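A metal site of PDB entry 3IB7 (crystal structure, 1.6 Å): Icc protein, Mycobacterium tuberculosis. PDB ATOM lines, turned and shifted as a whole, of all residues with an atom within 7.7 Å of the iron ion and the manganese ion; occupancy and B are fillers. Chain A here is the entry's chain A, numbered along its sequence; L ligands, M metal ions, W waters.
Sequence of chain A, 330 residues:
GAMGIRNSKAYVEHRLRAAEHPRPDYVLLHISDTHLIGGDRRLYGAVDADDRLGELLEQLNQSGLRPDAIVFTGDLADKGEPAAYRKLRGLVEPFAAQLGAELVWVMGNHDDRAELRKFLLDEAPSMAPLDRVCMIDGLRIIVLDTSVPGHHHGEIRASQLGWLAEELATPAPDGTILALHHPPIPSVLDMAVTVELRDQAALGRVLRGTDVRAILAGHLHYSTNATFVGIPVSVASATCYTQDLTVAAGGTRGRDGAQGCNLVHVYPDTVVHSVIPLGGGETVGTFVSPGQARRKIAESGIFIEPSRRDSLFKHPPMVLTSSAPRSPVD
OD2 of Asp 33 lies within hydrogen-bond range of N of His 219, at 2.9 Å. The backbone NH (N) of Asp 33 sits at hydrogen-bond distance from the backbone carbonyl oxygen (O) of Gly 74 (2.9 Å). O of Asp 33 is in hydrogen-bond range of SG of Cys 240. ND2 of Asn 109 is in hydrogen-bond range of ND1 of His 152 (2.9 Å). A ring nitrogen (ND1) of His 35 lies within hydrogen-bond range of the side-chain carboxylate (OD1) of Asp 78 (2.8 Å). The side-chain carboxylate (OD2) of Asp 111 lies within hydrogen-bond range of the backbone NH (N) of Asp 75 (2.9 Å). A ring nitrogen (ND1) of His 221 sits at hydrogen-bond distance from the backbone carbonyl oxygen of Tyr 241. A ring nitrogen (NE2) of His 219 lies within hydrogen-bond range of the backbone carbonyl oxygen of Val 195 (2.9 Å).
The iron ion is bound by water W1, OD1 of Asp 33, NE2 of His 35, NE2 of His 221, OD2 of Asp 75 and O1 of the ligand.
The manganese ion is bound by the side-chain amide oxygen (OD1) of Asn 109 (2.2 Å), water W1 (2.2 Å), the side-chain carboxylate (OD2) of Asp 75 (2.2 Å), an oxygen (O2) of the ligand (2.2 Å), a ring nitrogen (NE2) of His 181 (2.3 Å) and a ring nitrogen (ND1) of His 219 (2.3 Å).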
ATOM      1  N   SER A  32      23.062 -23.061  18.325  1.00  0.00           N
ATOM      2  CA  SER A  32      23.595 -23.331  19.665  1.00  0.00           C
ATOM      3  C   SER A  32      25.087 -23.043  19.761  1.00  0.00           C
ATOM      4  O   SER A  32      25.805 -23.085  18.756  1.00  0.00           O
ATOM      5  CB  SER A  32      23.341 -24.810  20.055  1.00  0.00           C
ATOM      6  OG  SER A  32      23.416 -25.000  21.461  1.00  0.00           O
ATOM      7  N   ASP A  33      25.529 -22.743  20.970  1.00  0.00           N
ATOM      8  CA  ASP A  33      26.960 -22.772  21.282  1.00  0.00           C
ATOM      9  C   ASP A  33      27.767 -21.849  20.377  1.00  0.00           C
ATOM     10  O   ASP A  33      28.708 -22.273  19.693  1.00  0.00           O
ATOM     11  CB  ASP A  33      27.456 -24.217  21.207  1.00  0.00           C
ATOM     12  CG  ASP A  33      26.940 -25.055  22.360  1.00  0.00           C
ATOM     13  OD1 ASP A  33      27.561 -24.952  23.440  1.00  0.00           O
ATOM     14  OD2 ASP A  33      25.924 -25.785  22.201  1.00  0.00           O
ATOM     15  N   THR A  34      27.365 -20.581  20.378  1.00  0.00           N
ATOM     16  CA  THR A  34      28.024 -19.553  19.580  1.00  0.00           C
ATOM     17  C   THR A  34      29.387 -19.154  20.170  1.00  0.00           C
ATOM     18  O   THR A  34      30.327 -18.861  19.429  1.00  0.00           O
ATOM     19  CB  THR A  34      27.112 -18.311  19.402  1.00  0.00           C
ATOM     20  OG1 THR A  34      26.599 -17.920  20.670  1.00  0.00           O
ATOM     21  CG2 THR A  34      25.919 -18.669  18.490  1.00  0.00           C
ATOM     22  N   HIS A  35      29.487 -19.170  21.508  1.00  0.00           N
ATOM     23  CA  HIS A  35      30.756 -18.938  22.221  1.00  0.00           C
ATOM     24  C   HIS A  35      31.479 -17.661  21.772  1.00  0.00           C
ATOM     25  O   HIS A  35      32.704 -17.664  21.594  1.00  0.00           O
ATOM     26  CB  HIS A  35      31.687 -20.157  22.095  1.00  0.00           C
ATOM     27  CG  HIS A  35      31.302 -21.314  22.958  1.00  0.00           C
ATOM     28  ND1 HIS A  35      31.789 -21.471  24.239  1.00  0.00           N
ATOM     29  CD2 HIS A  35      30.473 -22.358  22.732  1.00  0.00           C
ATOM     30  CE1 HIS A  35      31.280 -22.577  24.764  1.00  0.00           C
ATOM     31  NE2 HIS A  35      30.480 -23.132  23.879  1.00  0.00           N
ATOM     32  N   TYR A  44      39.723 -19.223  21.740  1.00  0.00           N
ATOM     33  CA  TYR A  44      40.798 -20.135  22.142  1.00  0.00           C
ATOM     34  C   TYR A  44      42.027 -19.992  21.238  1.00  0.00           C
ATOM     35  O   TYR A  44      42.808 -20.930  21.080  1.00  0.00           O
ATOM     36  CB  TYR A  44      40.320 -21.600  22.206  1.00  0.00           C
ATOM     37  CG  TYR A  44      39.009 -21.830  22.937  1.00  0.00           C
ATOM     38  CD1 TYR A  44      38.501 -20.898  23.856  1.00  0.00           C
ATOM     39  CD2 TYR A  44      38.285 -23.018  22.737  1.00  0.00           C
ATOM     40  CE1 TYR A  44      37.294 -21.127  24.537  1.00  0.00           C
ATOM     41  CE2 TYR A  44      37.089 -23.255  23.414  1.00  0.00           C
ATOM     42  CZ  TYR A  44      36.589 -22.308  24.300  1.00  0.00           C
ATOM     43  OH  TYR A  44      35.394 -22.551  24.944  1.00  0.00           O
ATOM     44  N   THR A  73      20.243 -22.466  21.940  1.00  0.00           N
ATOM     45  CA  THR A  73      20.284 -23.335  23.125  1.00  0.00           C
ATOM     46  C   THR A  73      21.576 -23.263  23.951  1.00  0.00           C
ATOM     47  O   THR A  73      22.144 -24.288  24.331  1.00  0.00           O
ATOM     48  CB  THR A  73      19.891 -24.786  22.785  1.00  0.00           C
ATOM     49  OG1 THR A  73      20.696 -25.266  21.686  1.00  0.00           O
ATOM     50  CG2 THR A  73      18.393 -24.859  22.413  1.00  0.00           C
ATOM     51  N   GLY A  74      22.023 -22.041  24.241  1.00  0.00           N
ATOM     52  CA  GLY A  74      23.032 -21.811  25.278  1.00  0.00           C
ATOM     53  C   GLY A  74      24.482 -21.756  24.839  1.00  0.00           C
ATOM     54  O   GLY A  74      24.835 -22.104  23.696  1.00  0.00           O
ATOM     55  N   ASP A  75      25.329 -21.327  25.785  1.00  0.00           N
ATOM     56  CA  ASP A  75      26.739 -21.008  25.522  1.00  0.00           C
ATOM     57  C   ASP A  75      26.836 -19.912  24.465  1.00  0.00           C
ATOM     58  O   ASP A  75      27.528 -20.036  23.441  1.00  0.00           O
ATOM     59  CB  ASP A  75      27.574 -22.249  25.180  1.00  0.00           C
ATOM     60  CG  ASP A  75      27.920 -23.088  26.402  1.00  0.00           C
ATOM     61  OD1 ASP A  75      27.558 -22.704  27.544  1.00  0.00           O
ATOM     62  OD2 ASP A  75      28.558 -24.144  26.240  1.00  0.00           O
ATOM     63  N   LEU A  76      26.108 -18.832  24.736  1.00  0.00           N
ATOM     64  CA  LEU A  76      26.020 -17.712  23.807  1.00  0.00           C
ATOM     65  C   LEU A  76      27.323 -16.914  23.815  1.00  0.00           C
ATOM     66  O   LEU A  76      27.901 -16.665  22.758  1.00  0.00           O
ATOM     67  CB  LEU A  76      24.807 -16.820  24.163  1.00  0.00           C
ATOM     68  CG  LEU A  76      23.493 -17.573  24.439  1.00  0.00           C
ATOM     69  CD1 LEU A  76      22.376 -16.634  24.915  1.00  0.00           C
ATOM     70  CD2 LEU A  76      23.064 -18.391  23.228  1.00  0.00           C
ATOM     71  N   ASP A  78      31.230 -16.983  25.384  1.00  0.00           N
ATOM     72  CA  ASP A  78      32.174 -17.965  25.927  1.00  0.00           C
ATOM     73  C   ASP A  78      32.587 -17.747  27.390  1.00  0.00           C
ATOM     74  O   ASP A  78      32.883 -18.708  28.096  1.00  0.00           O
ATOM     75  CB  ASP A  78      33.437 -18.048  25.088  1.00  0.00           C
ATOM     76  CG  ASP A  78      34.363 -19.124  25.583  1.00  0.00           C
ATOM     77  OD1 ASP A  78      34.009 -20.323  25.405  1.00  0.00           O
ATOM     78  OD2 ASP A  78      35.401 -18.790  26.178  1.00  0.00           O
ATOM     79  N   MET A 107      20.202 -20.062  28.512  1.00  0.00           N
ATOM     80  CA  MET A 107      21.492 -20.121  29.215  1.00  0.00           C
ATOM     81  C   MET A 107      22.268 -21.407  28.932  1.00  0.00           C
ATOM     82  O   MET A 107      21.696 -22.491  28.859  1.00  0.00           O
ATOM     83  CB  MET A 107      21.265 -20.082  30.739  1.00  0.00           C
ATOM     84  CG  MET A 107      21.058 -18.691  31.329  1.00  0.00           C
ATOM     85  SD  MET A 107      22.600 -17.735  31.428  1.00  0.00           S
ATOM     86  CE  MET A 107      23.652 -18.843  32.396  1.00  0.00           C
ATOM     87  N   GLY A 108      23.595 -21.277  28.791  1.00  0.00           N
ATOM     88  CA  GLY A 108      24.491 -22.418  28.850  1.00  0.00           C
ATOM     89  C   GLY A 108      25.483 -22.259  30.006  1.00  0.00           C
ATOM     90  O   GLY A 108      25.481 -21.226  30.686  1.00  0.00           O
ATOM     91  N   ASN A 109      26.312 -23.272  30.232  1.00  0.00           N
ATOM     92  CA  ASN A 109      27.294 -23.225  31.327  1.00  0.00           C
ATOM     93  C   ASN A 109      28.325 -22.083  31.225  1.00  0.00           C
ATOM     94  O   ASN A 109      28.851 -21.634  32.253  1.00  0.00           O
ATOM     95  CB  ASN A 109      27.984 -24.565  31.548  1.00  0.00           C
ATOM     96  CG  ASN A 109      28.604 -25.138  30.293  1.00  0.00           C
ATOM     97  OD1 ASN A 109      27.908 -25.388  29.296  1.00  0.00           O
ATOM     98  ND2 ASN A 109      29.918 -25.373  30.324  1.00  0.00           N
ATOM     99  N   HIS A 110      28.603 -21.615  30.002  1.00  0.00           N
ATOM    100  CA  HIS A 110      29.565 -20.531  29.774  1.00  0.00           C
ATOM    101  C   HIS A 110      28.944 -19.148  29.992  1.00  0.00           C
ATOM    102  O   HIS A 110      29.669 -18.160  30.165  1.00  0.00           O
ATOM    103  CB  HIS A 110      30.143 -20.613  28.362  1.00  0.00           C
ATOM    104  CG  HIS A 110      31.173 -21.697  28.214  1.00  0.00           C
ATOM    105  ND1 HIS A 110      32.502 -21.421  27.976  1.00  0.00           N
ATOM    106  CD2 HIS A 110      31.076 -23.041  28.280  1.00  0.00           C
ATOM    107  CE1 HIS A 110      33.177 -22.561  27.908  1.00  0.00           C
ATOM    108  NE2 HIS A 110      32.332 -23.550  28.097  1.00  0.00           N
ATOM    109  N   ASP A 111      27.617 -19.074  29.988  1.00  0.00           N
ATOM    110  CA  ASP A 111      26.953 -17.774  30.143  1.00  0.00           C
ATOM    111  C   ASP A 111      26.925 -17.290  31.586  1.00  0.00           C
ATOM    112  O   ASP A 111      27.117 -18.063  32.509  1.00  0.00           O
ATOM    113  CB  ASP A 111      25.533 -17.837  29.569  1.00  0.00           C
ATOM    114  CG  ASP A 111      25.540 -17.985  28.069  1.00  0.00           C
ATOM    115  OD1 ASP A 111      25.981 -17.036  27.381  1.00  0.00           O
ATOM    116  OD2 ASP A 111      25.124 -19.063  27.594  1.00  0.00           O
ATOM    117  N   HIS A 152      30.270 -26.286  35.468  1.00  0.00           N
ATOM    118  CA  HIS A 152      30.044 -26.617  34.057  1.00  0.00           C
ATOM    119  C   HIS A 152      29.110 -27.784  33.767  1.00  0.00           C
ATOM    120  O   HIS A 152      28.604 -27.913  32.650  1.00  0.00           O
ATOM    121  CB  HIS A 152      31.380 -26.759  33.347  1.00  0.00           C
ATOM    122  CG  HIS A 152      32.120 -25.470  33.317  1.00  0.00           C
ATOM    123  ND1 HIS A 152      31.875 -24.516  32.352  1.00  0.00           N
ATOM    124  CD2 HIS A 152      32.999 -24.927  34.187  1.00  0.00           C
ATOM    125  CE1 HIS A 152      32.621 -23.456  32.601  1.00  0.00           C
ATOM    126  NE2 HIS A 152      33.302 -23.675  33.709  1.00  0.00           N
ATOM    127  N   HIS A 181      20.104 -26.280  27.748  1.00  0.00           N
ATOM    128  CA  HIS A 181      21.470 -26.453  27.266  1.00  0.00           C
ATOM    129  C   HIS A 181      21.974 -27.899  27.379  1.00  0.00           C
ATOM    130  O   HIS A 181      22.325 -28.526  26.361  1.00  0.00           O
ATOM    131  CB  HIS A 181      22.431 -25.509  27.994  1.00  0.00           C
ATOM    132  CG  HIS A 181      23.815 -25.515  27.442  1.00  0.00           C
ATOM    133  ND1 HIS A 181      24.098 -25.103  26.152  1.00  0.00           N
ATOM    134  CD2 HIS A 181      24.999 -25.879  27.993  1.00  0.00           C
ATOM    135  CE1 HIS A 181      25.394 -25.202  25.940  1.00  0.00           C
ATOM    136  NE2 HIS A 181      25.963 -25.676  27.042  1.00  0.00           N
ATOM    137  N   HIS A 182      22.053 -28.393  28.620  1.00  0.00           N
ATOM    138  CA  HIS A 182      22.585 -29.740  28.887  1.00  0.00           C
ATOM    139  C   HIS A 182      21.530 -30.801  28.559  1.00  0.00           C
ATOM    140  O   HIS A 182      20.466 -30.833  29.205  1.00  0.00           O
ATOM    141  CB  HIS A 182      22.959 -29.904  30.374  1.00  0.00           C
ATOM    142  CG  HIS A 182      24.058 -29.004  30.850  1.00  0.00           C
ATOM    143  ND1 HIS A 182      23.855 -27.692  31.208  1.00  0.00           N
ATOM    144  CD2 HIS A 182      25.366 -29.263  31.100  1.00  0.00           C
ATOM    145  CE1 HIS A 182      24.991 -27.166  31.619  1.00  0.00           C
ATOM    146  NE2 HIS A 182      25.928 -28.097  31.575  1.00  0.00           N
ATOM    147  N   VAL A 195      30.681 -33.171  32.724  1.00  0.00           N
ATOM    148  CA  VAL A 195      29.884 -31.947  32.632  1.00  0.00           C
ATOM    149  C   VAL A 195      28.446 -32.209  32.146  1.00  0.00           C
ATOM    150  O   VAL A 195      27.780 -31.307  31.627  1.00  0.00           O
ATOM    151  CB  VAL A 195      30.588 -30.871  31.756  1.00  0.00           C
ATOM    152  CG1 VAL A 195      31.847 -30.324  32.457  1.00  0.00           C
ATOM    153  CG2 VAL A 195      30.946 -31.436  30.375  1.00  0.00           C
ATOM    154  N   GLY A 218      21.899 -28.328  23.409  1.00  0.00           N
ATOM    155  CA  GLY A 218      23.204 -28.083  22.799  1.00  0.00           C
ATOM    156  C   GLY A 218      24.271 -28.785  23.633  1.00  0.00           C
ATOM    157  O   GLY A 218      24.134 -29.976  23.934  1.00  0.00           O
ATOM    158  N   HIS A 219      25.329 -28.046  23.972  1.00  0.00           N
ATOM    159  CA  HIS A 219      26.378 -28.459  24.922  1.00  0.00           C
ATOM    160  C   HIS A 219      27.391 -29.474  24.362  1.00  0.00           C
ATOM    161  O   HIS A 219      28.583 -29.367  24.660  1.00  0.00           O
ATOM    162  CB  HIS A 219      25.750 -28.953  26.243  1.00  0.00           C
ATOM    163  CG  HIS A 219      26.721 -29.189  27.357  1.00  0.00           C
ATOM    164  ND1 HIS A 219      27.596 -28.237  27.832  1.00  0.00           N
ATOM    165  CD2 HIS A 219      26.888 -30.278  28.160  1.00  0.00           C
ATOM    166  CE1 HIS A 219      28.286 -28.726  28.840  1.00  0.00           C
ATOM    167  NE2 HIS A 219      27.880 -29.970  29.068  1.00  0.00           N
ATOM    168  N   LEU A 220      26.936 -30.428  23.544  1.00  0.00           N
ATOM    169  CA  LEU A 220      27.832 -31.490  23.093  1.00  0.00           C
ATOM    170  C   LEU A 220      28.744 -31.101  21.929  1.00  0.00           C
ATOM    171  O   LEU A 220      29.775 -31.758  21.717  1.00  0.00           O
ATOM    172  CB  LEU A 220      27.041 -32.767  22.785  1.00  0.00           C
ATOM    173  CG  LEU A 220      26.368 -33.404  24.022  1.00  0.00           C
ATOM    174  CD1 LEU A 220      25.506 -34.594  23.625  1.00  0.00           C
ATOM    175  CD2 LEU A 220      27.382 -33.841  25.073  1.00  0.00           C
ATOM    176  N   HIS A 221      28.358 -30.060  21.171  1.00  0.00           N
ATOM    177  CA  HIS A 221      29.145 -29.615  20.010  1.00  0.00           C
ATOM    178  C   HIS A 221      29.284 -30.710  18.945  1.00  0.00           C
ATOM    179  O   HIS A 221      30.293 -30.780  18.246  1.00  0.00           O
ATOM    180  CB  HIS A 221      30.533 -29.098  20.428  1.00  0.00           C
ATOM    181  CG  HIS A 221      30.510 -27.787  21.166  1.00  0.00           C
ATOM    182  ND1 HIS A 221      31.281 -26.709  20.783  1.00  0.00           N
ATOM    183  CD2 HIS A 221      29.840 -27.391  22.271  1.00  0.00           C
ATOM    184  CE1 HIS A 221      31.082 -25.705  21.618  1.00  0.00           C
ATOM    185  NE2 HIS A 221      30.218 -26.098  22.533  1.00  0.00           N
ATOM    186  N   ALA A 238      27.520 -26.970  17.147  1.00  0.00           N
ATOM    187  CA  ALA A 238      27.928 -25.609  17.513  1.00  0.00           C
ATOM    188  C   ALA A 238      28.240 -24.771  16.277  1.00  0.00           C
ATOM    189  O   ALA A 238      28.574 -25.317  15.223  1.00  0.00           O
ATOM    190  CB  ALA A 238      29.170 -25.664  18.420  1.00  0.00           C
ATOM    191  N   CYS A 240      30.674 -22.391  16.408  1.00  0.00           N
ATOM    192  CA  CYS A 240      32.077 -21.987  16.526  1.00  0.00           C
ATOM    193  C   CYS A 240      33.088 -23.075  16.151  1.00  0.00           C
ATOM    194  O   CYS A 240      33.946 -22.868  15.282  1.00  0.00           O
ATOM    195  CB  CYS A 240      32.369 -21.451  17.929  1.00  0.00           C
ATOM    196  SG  CYS A 240      31.913 -22.573  19.275  1.00  0.00           S
ATOM    197  N   TYR A 241      32.991 -24.231  16.808  1.00  0.00           N
ATOM    198  CA  TYR A 241      33.865 -25.375  16.535  1.00  0.00           C
ATOM    199  C   TYR A 241      33.096 -26.622  16.977  1.00  0.00           C
ATOM    200  O   TYR A 241      32.206 -26.532  17.814  1.00  0.00           O
ATOM    201  CB  TYR A 241      35.208 -25.261  17.287  1.00  0.00           C
ATOM    202  CG  TYR A 241      35.067 -25.574  18.756  1.00  0.00           C
ATOM    203  CD1 TYR A 241      35.221 -26.895  19.233  1.00  0.00           C
ATOM    204  CD2 TYR A 241      34.757 -24.577  19.684  1.00  0.00           C
ATOM    205  CE1 TYR A 241      35.070 -27.195  20.579  1.00  0.00           C
ATOM    206  CE2 TYR A 241      34.589 -24.875  21.032  1.00  0.00           C
ATOM    207  CZ  TYR A 241      34.751 -26.181  21.476  1.00  0.00           C
ATOM    208  OH  TYR A 241      34.592 -26.497  22.810  1.00  0.00           O
HETATM  209  C1  LIG L   1      31.381 -26.136  26.785  1.00  0.00           C
HETATM  210  O1  LIG L   1      31.237 -25.479  25.716  1.00  0.00           O
HETATM  211  O2  LIG L   1      30.389 -26.240  27.563  1.00  0.00           O
HETATM  212  C2  LIG L   1      32.698 -26.750  27.101  1.00  0.00           C
HETATM  213 FE    FE M   1      29.464 -25.032  24.362  1.00  0.00          FE
HETATM  214 MN    MN M   2      28.167 -26.091  27.263  1.00  0.00          MN
HETATM  215  O   HOH W   1      28.854 -26.730  25.242  1.00  0.00           O
